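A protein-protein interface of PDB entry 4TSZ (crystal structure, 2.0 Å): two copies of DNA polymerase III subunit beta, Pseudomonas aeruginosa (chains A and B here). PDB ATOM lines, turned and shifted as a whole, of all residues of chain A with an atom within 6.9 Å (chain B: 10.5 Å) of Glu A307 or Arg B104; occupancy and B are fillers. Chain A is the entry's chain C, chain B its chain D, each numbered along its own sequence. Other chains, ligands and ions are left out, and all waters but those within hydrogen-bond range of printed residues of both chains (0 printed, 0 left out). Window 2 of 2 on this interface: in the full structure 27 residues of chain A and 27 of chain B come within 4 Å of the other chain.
The guanidinium group (NH2) of Arg A271 lies within salt-bridge range of the side-chain carboxylate (OE1) of Glu A306, at 2.7 Å. O of Glu A306 is in hydrogen-bond range of N of Ile A294, at 2.7 Å. The backbone carbonyl oxygen of Val B100 is in hydrogen-bond range of the backbone NH of Phe B107, 2.8 Å away.
NE of Arg A271 is in hydrogen-bond range of OG of Ser B105, at 3.4 Å. N of Glu A305 lies within hydrogen-bond range of O of Arg B106, at 2.9 Å. The side-chain carboxylate (OE2) of Glu A306 sits at hydrogen-bond distance from the side-chain hydroxyl (OG) of Ser B105, at 3.2 Å. The side-chain carboxylate (OE1) of Glu A307 lies within salt-bridge range of the guanidinium group (NH1) of Arg B104, 2.8 Å away.
Arg B104 touches just these residues of chain A: Leu A291 (3.7 Å), Glu A305 (3.9 Å), Glu A306 (3.6 Å), Glu A307 (2.8 Å) and Gln A309 (3.6 Å). Of chain B, only Arg B104 (3.6 Å) and Ser B105 (3.2 Å) come within 4 Å of Glu A306. No residue of chain B comes within 4 Å of Val A308. Of the printed residues of chain A, Ser B105 touches Arg A271, Glu A305 and Glu A306. Printed residues of chain A within 4 Å of Arg B106: Glu A305. Ile B89 touches none of the printed residues of chain A. The nearest residue of chain A that does not touch Arg B104 is Val A308 (4.2 Å).
No position is printed for both chains.
Among the printed residues, pairs that only touch across the chains: Gln A309 with Arg B104 (3.6 Å), Glu A306 with Arg B104 (3.6 Å), Glu A305 with Ser B105 (3.6 Å), Arg A271 with Pro B84 (3.7 Å), Arg A271 with Phe B107 (3.7 Å), Leu A291 with Arg B104 (3.7 Å), Arg A271 with Leu B83 (3.8 Å) and Glu A305 with Arg B104 (3.9 Å).
Printed residues of chain B that touch a printed residue of chain A: Leu B83, Pro B84, Arg B104, Ser B105, Arg B106 and Phe B107. Hydrophobic or aromatic side chains of chain B within 4 Å of the printed part of chain A: Leu B83, Pro B84 and Phe B107. Of the 14 printed residues of chain A, 6 touch a printed residue of chain B. Hydrophobic or aromatic side chains of chain A that line the printed part of chain B: Leu A291. Along chain A the printed residues that touch a printed residue of chain B span positions 271 to 309. Among the printed residues, Asp or Glu carboxylates within 4 Å of a Lys or Arg side-chain nitrogen of the other chain: Glu A307 with Arg B104.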
ATOM      1  N   GLN A 264     -24.469 -30.406  16.027  1.00  0.00           N
ATOM      2  CA  GLN A 264     -24.652 -29.234  15.163  1.00  0.00           C
ATOM      3  C   GLN A 264     -25.641 -28.249  15.785  1.00  0.00           C
ATOM      4  O   GLN A 264     -25.380 -27.050  15.788  1.00  0.00           O
ATOM      5  CB  GLN A 264     -25.142 -29.647  13.771  1.00  0.00           C
ATOM      6  CG  GLN A 264     -24.070 -30.243  12.871  1.00  0.00           C
ATOM      7  CD  GLN A 264     -24.559 -30.288  11.445  1.00  0.00           C
ATOM      8  OE1 GLN A 264     -25.422 -31.087  11.079  1.00  0.00           O
ATOM      9  NE2 GLN A 264     -24.054 -29.391  10.618  1.00  0.00           N
ATOM     10  N   ALA A 268     -24.647 -24.490  17.288  1.00  0.00           N
ATOM     11  CA  ALA A 268     -25.356 -23.330  16.740  1.00  0.00           C
ATOM     12  C   ALA A 268     -26.134 -22.589  17.824  1.00  0.00           C
ATOM     13  O   ALA A 268     -26.122 -21.356  17.833  1.00  0.00           O
ATOM     14  CB  ALA A 268     -26.295 -23.770  15.631  1.00  0.00           C
ATOM     15  N   ARG A 271     -23.512 -20.714  20.022  1.00  0.00           N
ATOM     16  CA  ARG A 271     -22.986 -19.526  19.322  1.00  0.00           C
ATOM     17  C   ARG A 271     -23.982 -18.379  19.368  1.00  0.00           C
ATOM     18  O   ARG A 271     -23.607 -17.271  19.753  1.00  0.00           O
ATOM     19  CB  ARG A 271     -22.610 -19.834  17.870  1.00  0.00           C
ATOM     20  CG  ARG A 271     -21.320 -20.629  17.731  1.00  0.00           C
ATOM     21  CD  ARG A 271     -20.855 -20.746  16.301  1.00  0.00           C
ATOM     22  NE  ARG A 271     -21.599 -21.758  15.551  1.00  0.00           N
ATOM     23  CZ  ARG A 271     -21.225 -23.024  15.432  1.00  0.00           C
ATOM     24  NH1 ARG A 271     -20.124 -23.458  16.030  1.00  0.00           N
ATOM     25  NH2 ARG A 271     -21.947 -23.868  14.713  1.00  0.00           N
ATOM     26  N   GLY A 290     -35.794 -28.787   5.007  1.00  0.00           N
ATOM     27  CA  GLY A 290     -34.390 -29.113   5.240  1.00  0.00           C
ATOM     28  C   GLY A 290     -33.554 -28.066   5.955  1.00  0.00           C
ATOM     29  O   GLY A 290     -32.328 -28.195   6.002  1.00  0.00           O
ATOM     30  N   LEU A 291     -34.192 -27.028   6.530  1.00  0.00           N
ATOM     31  CA  LEU A 291     -33.454 -25.925   7.134  1.00  0.00           C
ATOM     32  C   LEU A 291     -34.026 -25.351   8.422  1.00  0.00           C
ATOM     33  O   LEU A 291     -35.227 -25.126   8.533  1.00  0.00           O
ATOM     34  CB  LEU A 291     -33.294 -24.811   6.064  1.00  0.00           C
ATOM     35  CG  LEU A 291     -32.490 -23.549   6.402  1.00  0.00           C
ATOM     36  CD1 LEU A 291     -31.000 -23.853   6.538  1.00  0.00           C
ATOM     37  CD2 LEU A 291     -32.709 -22.484   5.349  1.00  0.00           C
ATOM     38  N   LEU A 292     -33.132 -25.063   9.376  1.00  0.00           N
ATOM     39  CA  LEU A 292     -33.464 -24.378  10.618  1.00  0.00           C
ATOM     40  C   LEU A 292     -32.607 -23.110  10.735  1.00  0.00           C
ATOM     41  O   LEU A 292     -31.384 -23.195  10.888  1.00  0.00           O
ATOM     42  CB  LEU A 292     -33.315 -25.277  11.867  1.00  0.00           C
ATOM     43  CG  LEU A 292     -33.764 -24.626  13.192  1.00  0.00           C
ATOM     44  CD1 LEU A 292     -35.286 -24.533  13.282  1.00  0.00           C
ATOM     45  CD2 LEU A 292     -33.213 -25.371  14.384  1.00  0.00           C
ATOM     46  N   LYS A 293     -33.255 -21.941  10.629  1.00  0.00           N
ATOM     47  CA  LYS A 293     -32.586 -20.647  10.777  1.00  0.00           C
ATOM     48  C   LYS A 293     -32.733 -20.226  12.240  1.00  0.00           C
ATOM     49  O   LYS A 293     -33.841 -20.284  12.782  1.00  0.00           O
ATOM     50  CB  LYS A 293     -33.203 -19.580   9.857  1.00  0.00           C
ATOM     51  CG  LYS A 293     -32.982 -19.801   8.363  1.00  0.00           C
ATOM     52  CD  LYS A 293     -33.591 -18.647   7.570  1.00  0.00           C
ATOM     53  CE  LYS A 293     -33.628 -18.884   6.081  1.00  0.00           C
ATOM     54  NZ  LYS A 293     -34.212 -17.726   5.355  1.00  0.00           N
ATOM     55  N   ILE A 294     -31.613 -19.855  12.886  1.00  0.00           N
ATOM     56  CA  ILE A 294     -31.582 -19.423  14.282  1.00  0.00           C
ATOM     57  C   ILE A 294     -31.123 -17.974  14.365  1.00  0.00           C
ATOM     58  O   ILE A 294     -30.103 -17.612  13.776  1.00  0.00           O
ATOM     59  CB  ILE A 294     -30.718 -20.349  15.185  1.00  0.00           C
ATOM     60  CG1 ILE A 294     -31.032 -21.840  14.941  1.00  0.00           C
ATOM     61  CG2 ILE A 294     -30.857 -19.969  16.693  1.00  0.00           C
ATOM     62  CD1 ILE A 294     -29.878 -22.747  15.184  1.00  0.00           C
ATOM     63  N   GLU A 305     -26.768 -14.908  13.943  1.00  0.00           N
ATOM     64  CA  GLU A 305     -27.563 -15.675  12.985  1.00  0.00           C
ATOM     65  C   GLU A 305     -26.830 -16.921  12.550  1.00  0.00           C
ATOM     66  O   GLU A 305     -25.614 -16.892  12.345  1.00  0.00           O
ATOM     67  CB  GLU A 305     -27.936 -14.835  11.752  1.00  0.00           C
ATOM     68  CG  GLU A 305     -29.010 -13.793  12.012  1.00  0.00           C
ATOM     69  CD  GLU A 305     -29.516 -13.041  10.796  1.00  0.00           C
ATOM     70  OE1 GLU A 305     -30.714 -12.680  10.784  1.00  0.00           O
ATOM     71  OE2 GLU A 305     -28.716 -12.797   9.865  1.00  0.00           O
ATOM     72  N   GLU A 306     -27.575 -18.018  12.401  1.00  0.00           N
ATOM     73  CA  GLU A 306     -27.036 -19.288  11.939  1.00  0.00           C
ATOM     74  C   GLU A 306     -28.089 -20.123  11.227  1.00  0.00           C
ATOM     75  O   GLU A 306     -29.276 -20.030  11.533  1.00  0.00           O
ATOM     76  CB  GLU A 306     -26.372 -20.076  13.081  1.00  0.00           C
ATOM     77  CG  GLU A 306     -25.209 -20.901  12.551  1.00  0.00           C
ATOM     78  CD  GLU A 306     -24.315 -21.576  13.567  1.00  0.00           C
ATOM     79  OE1 GLU A 306     -23.942 -22.748  13.328  1.00  0.00           O
ATOM     80  OE2 GLU A 306     -23.957 -20.930  14.577  1.00  0.00           O
ATOM     81  N   GLU A 307     -27.642 -20.920  10.260  1.00  0.00           N
ATOM     82  CA  GLU A 307     -28.490 -21.811   9.485  1.00  0.00           C
ATOM     83  C   GLU A 307     -27.979 -23.228   9.700  1.00  0.00           C
ATOM     84  O   GLU A 307     -26.777 -23.482   9.556  1.00  0.00           O
ATOM     85  CB  GLU A 307     -28.457 -21.441   7.996  1.00  0.00           C
ATOM     86  CG  GLU A 307     -29.118 -20.115   7.668  1.00  0.00           C
ATOM     87  CD  GLU A 307     -29.265 -19.821   6.186  1.00  0.00           C
ATOM     88  OE1 GLU A 307     -28.326 -20.122   5.413  1.00  0.00           O
ATOM     89  OE2 GLU A 307     -30.317 -19.264   5.800  1.00  0.00           O
ATOM     90  N   VAL A 308     -28.884 -24.133  10.109  1.00  0.00           N
ATOM     91  CA  VAL A 308     -28.568 -25.537  10.366  1.00  0.00           C
ATOM     92  C   VAL A 308     -29.412 -26.425   9.453  1.00  0.00           C
ATOM     93  O   VAL A 308     -30.638 -26.273   9.403  1.00  0.00           O
ATOM     94  CB  VAL A 308     -28.737 -25.930  11.863  1.00  0.00           C
ATOM     95  CG1 VAL A 308     -28.322 -27.380  12.109  1.00  0.00           C
ATOM     96  CG2 VAL A 308     -27.958 -24.990  12.775  1.00  0.00           C
ATOM     97  N   GLN A 309     -28.756 -27.357   8.751  1.00  0.00           N
ATOM     98  CA  GLN A 309     -29.447 -28.322   7.899  1.00  0.00           C
ATOM     99  C   GLN A 309     -30.102 -29.363   8.798  1.00  0.00           C
ATOM    100  O   GLN A 309     -29.468 -29.869   9.723  1.00  0.00           O
ATOM    101  CB  GLN A 309     -28.487 -28.980   6.896  1.00  0.00           C
ATOM    102  CG  GLN A 309     -28.251 -28.149   5.646  1.00  0.00           C
ATOM    103  CD  GLN A 309     -27.377 -28.881   4.667  1.00  0.00           C
ATOM    104  OE1 GLN A 309     -26.154 -28.712   4.644  1.00  0.00           O
ATOM    105  NE2 GLN A 309     -27.982 -29.725   3.842  1.00  0.00           N
ATOM    106  N   VAL A 310     -31.393 -29.622   8.577  1.00  0.00           N
ATOM    107  CA  VAL A 310     -32.178 -30.588   9.357  1.00  0.00           C
ATOM    108  C   VAL A 310     -32.989 -31.480   8.406  1.00  0.00           C
ATOM    109  O   VAL A 310     -33.195 -31.100   7.259  1.00  0.00           O
ATOM    110  CB  VAL A 310     -33.107 -29.896  10.405  1.00  0.00           C
ATOM    111  CG1 VAL A 310     -32.310 -29.214  11.523  1.00  0.00           C
ATOM    112  CG2 VAL A 310     -34.092 -28.920   9.753  1.00  0.00           C
ATOM    113  N   LEU B  83     -16.671 -21.059  17.676  1.00  0.00           N
ATOM    114  CA  LEU B  83     -16.626 -21.325  16.238  1.00  0.00           C
ATOM    115  C   LEU B  83     -15.965 -22.675  15.920  1.00  0.00           C
ATOM    116  O   LEU B  83     -15.149 -23.131  16.725  1.00  0.00           O
ATOM    117  CB  LEU B  83     -15.944 -20.175  15.487  1.00  0.00           C
ATOM    118  CG  LEU B  83     -16.794 -18.924  15.268  1.00  0.00           C
ATOM    119  CD1 LEU B  83     -15.940 -17.777  14.775  1.00  0.00           C
ATOM    120  CD2 LEU B  83     -17.956 -19.184  14.324  1.00  0.00           C
ATOM    121  N   PRO B  84     -16.329 -23.357  14.800  1.00  0.00           N
ATOM    122  CA  PRO B  84     -15.690 -24.655  14.489  1.00  0.00           C
ATOM    123  C   PRO B  84     -14.175 -24.540  14.318  1.00  0.00           C
ATOM    124  O   PRO B  84     -13.684 -23.531  13.797  1.00  0.00           O
ATOM    125  CB  PRO B  84     -16.352 -25.084  13.172  1.00  0.00           C
ATOM    126  CG  PRO B  84     -17.588 -24.278  13.071  1.00  0.00           C
ATOM    127  CD  PRO B  84     -17.296 -22.980  13.746  1.00  0.00           C
ATOM    128  N   VAL B  87     -11.740 -22.688  11.288  1.00  0.00           N
ATOM    129  CA  VAL B  87     -12.546 -21.846  10.395  1.00  0.00           C
ATOM    130  C   VAL B  87     -11.865 -20.481  10.101  1.00  0.00           C
ATOM    131  O   VAL B  87     -11.155 -19.935  10.957  1.00  0.00           O
ATOM    132  CB  VAL B  87     -14.019 -21.707  10.894  1.00  0.00           C
ATOM    133  CG1 VAL B  87     -14.147 -20.735  12.075  1.00  0.00           C
ATOM    134  CG2 VAL B  87     -14.960 -21.317   9.758  1.00  0.00           C
ATOM    135  N   LEU B  88     -12.077 -19.954   8.886  1.00  0.00           N
ATOM    136  CA  LEU B  88     -11.569 -18.635   8.511  1.00  0.00           C
ATOM    137  C   LEU B  88     -12.632 -17.607   8.915  1.00  0.00           C
ATOM    138  O   LEU B  88     -13.801 -17.734   8.530  1.00  0.00           O
ATOM    139  CB  LEU B  88     -11.261 -18.552   7.004  1.00  0.00           C
ATOM    140  CG  LEU B  88     -10.589 -17.260   6.513  1.00  0.00           C
ATOM    141  CD1 LEU B  88      -9.160 -17.138   7.030  1.00  0.00           C
ATOM    142  CD2 LEU B  88     -10.586 -17.196   4.999  1.00  0.00           C
ATOM    143  N   ILE B  89     -12.234 -16.618   9.715  1.00  0.00           N
ATOM    144  CA  ILE B  89     -13.142 -15.580  10.203  1.00  0.00           C
ATOM    145  C   ILE B  89     -12.949 -14.283   9.415  1.00  0.00           C
ATOM    146  O   ILE B  89     -11.827 -13.788   9.311  1.00  0.00           O
ATOM    147  CB  ILE B  89     -12.985 -15.353  11.739  1.00  0.00           C
ATOM    148  CG1 ILE B  89     -13.025 -16.686  12.535  1.00  0.00           C
ATOM    149  CG2 ILE B  89     -14.018 -14.348  12.261  1.00  0.00           C
ATOM    150  CD1 ILE B  89     -12.453 -16.588  13.960  1.00  0.00           C
ATOM    151  N   ASP B  90     -14.048 -13.734   8.880  1.00  0.00           N
ATOM    152  CA  ASP B  90     -14.032 -12.456   8.190  1.00  0.00           C
ATOM    153  C   ASP B  90     -14.558 -11.403   9.166  1.00  0.00           C
ATOM    154  O   ASP B  90     -15.663 -11.543   9.704  1.00  0.00           O
ATOM    155  CB  ASP B  90     -14.864 -12.495   6.898  1.00  0.00           C
ATOM    156  CG  ASP B  90     -14.698 -11.233   6.075  1.00  0.00           C
ATOM    157  OD1 ASP B  90     -15.331 -10.211   6.419  1.00  0.00           O
ATOM    158  OD2 ASP B  90     -13.901 -11.250   5.119  1.00  0.00           O
ATOM    159  N   VAL B 100     -18.930 -10.015  11.973  1.00  0.00           N
ATOM    160  CA  VAL B 100     -18.148 -11.249  12.056  1.00  0.00           C
ATOM    161  C   VAL B 100     -18.846 -12.331  11.230  1.00  0.00           C
ATOM    162  O   VAL B 100     -20.026 -12.604  11.454  1.00  0.00           O
ATOM    163  CB  VAL B 100     -17.931 -11.686  13.536  1.00  0.00           C
ATOM    164  CG1 VAL B 100     -17.057 -12.934  13.634  1.00  0.00           C
ATOM    165  CG2 VAL B 100     -17.339 -10.558  14.374  1.00  0.00           C
ATOM    166  N   LYS B 101     -18.122 -12.927  10.270  1.00  0.00           N
ATOM    167  CA  LYS B 101     -18.620 -14.003   9.404  1.00  0.00           C
ATOM    168  C   LYS B 101     -17.656 -15.184   9.448  1.00  0.00           C
ATOM    169  O   LYS B 101     -16.450 -15.002   9.296  1.00  0.00           O
ATOM    170  CB  LYS B 101     -18.780 -13.526   7.948  1.00  0.00           C
ATOM    171  CG  LYS B 101     -19.956 -12.598   7.695  1.00  0.00           C
ATOM    172  CD  LYS B 101     -19.987 -12.160   6.233  1.00  0.00           C
ATOM    173  N   ALA B 102     -18.182 -16.392   9.671  1.00  0.00           N
ATOM    174  CA  ALA B 102     -17.389 -17.618   9.706  1.00  0.00           C
ATOM    175  C   ALA B 102     -18.300 -18.786   9.363  1.00  0.00           C
ATOM    176  O   ALA B 102     -19.205 -19.138  10.137  1.00  0.00           O
ATOM    177  CB  ALA B 102     -16.742 -17.807  11.070  1.00  0.00           C
ATOM    178  N   GLY B 103     -18.082 -19.339   8.173  1.00  0.00           N
ATOM    179  CA  GLY B 103     -18.893 -20.418   7.638  1.00  0.00           C
ATOM    180  C   GLY B 103     -20.322 -19.952   7.477  1.00  0.00           C
ATOM    181  O   GLY B 103     -20.566 -18.906   6.865  1.00  0.00           O
ATOM    182  N   ARG B 104     -21.259 -20.671   8.115  1.00  0.00           N
ATOM    183  CA  ARG B 104     -22.683 -20.330   8.077  1.00  0.00           C
ATOM    184  C   ARG B 104     -23.127 -19.470   9.282  1.00  0.00           C
ATOM    185  O   ARG B 104     -24.326 -19.244   9.475  1.00  0.00           O
ATOM    186  CB  ARG B 104     -23.533 -21.592   7.907  1.00  0.00           C
ATOM    187  CG  ARG B 104     -23.368 -22.234   6.516  1.00  0.00           C
ATOM    188  CD  ARG B 104     -24.663 -22.291   5.727  1.00  0.00           C
ATOM    189  NE  ARG B 104     -25.477 -23.452   6.104  1.00  0.00           N
ATOM    190  CZ  ARG B 104     -26.737 -23.653   5.726  1.00  0.00           C
ATOM    191  NH1 ARG B 104     -27.361 -22.762   4.963  1.00  0.00           N
ATOM    192  NH2 ARG B 104     -27.390 -24.736   6.125  1.00  0.00           N
ATOM    193  N   SER B 105     -22.152 -18.963  10.063  1.00  0.00           N
ATOM    194  CA  SER B 105     -22.405 -18.120  11.236  1.00  0.00           C
ATOM    195  C   SER B 105     -22.128 -16.643  10.945  1.00  0.00           C
ATOM    196  O   SER B 105     -21.127 -16.302  10.305  1.00  0.00           O
ATOM    197  CB  SER B 105     -21.569 -18.579  12.426  1.00  0.00           C
ATOM    198  OG  SER B 105     -21.606 -19.987  12.592  1.00  0.00           O
ATOM    199  N   ARG B 106     -23.032 -15.772  11.412  1.00  0.00           N
ATOM    200  CA  ARG B 106     -22.948 -14.318  11.263  1.00  0.00           C
ATOM    201  C   ARG B 106     -23.193 -13.664  12.618  1.00  0.00           C
ATOM    202  O   ARG B 106     -24.106 -14.072  13.336  1.00  0.00           O
ATOM    203  CB  ARG B 106     -23.963 -13.810  10.223  1.00  0.00           C
ATOM    204  CG  ARG B 106     -23.598 -14.173   8.784  1.00  0.00           C
ATOM    205  CD  ARG B 106     -24.703 -13.850   7.790  1.00  0.00           C
ATOM    206  NE  ARG B 106     -24.674 -12.448   7.364  1.00  0.00           N
ATOM    207  CZ  ARG B 106     -24.047 -12.000   6.277  1.00  0.00           C
ATOM    208  NH1 ARG B 106     -23.385 -12.840   5.489  1.00  0.00           N
ATOM    209  NH2 ARG B 106     -24.076 -10.710   5.972  1.00  0.00           N
ATOM    210  N   PHE B 107     -22.361 -12.673  12.977  1.00  0.00           N
ATOM    211  CA  PHE B 107     -22.458 -11.944  14.243  1.00  0.00           C
ATOM    212  C   PHE B 107     -22.295 -10.449  14.018  1.00  0.00           C
ATOM    213  O   PHE B 107     -21.439 -10.024  13.226  1.00  0.00           O
ATOM    214  CB  PHE B 107     -21.390 -12.418  15.254  1.00  0.00           C
ATOM    215  CG  PHE B 107     -21.339 -13.905  15.499  1.00  0.00           C
ATOM    216  CD1 PHE B 107     -20.572 -14.736  14.686  1.00  0.00           C
ATOM    217  CD2 PHE B 107     -22.049 -14.478  16.546  1.00  0.00           C
ATOM    218  CE1 PHE B 107     -20.532 -16.113  14.904  1.00  0.00           C
ATOM    219  CE2 PHE B 107     -22.002 -15.859  16.770  1.00  0.00           C
ATOM    220  CZ  PHE B 107     -21.248 -16.668  15.943  1.00  0.00           C
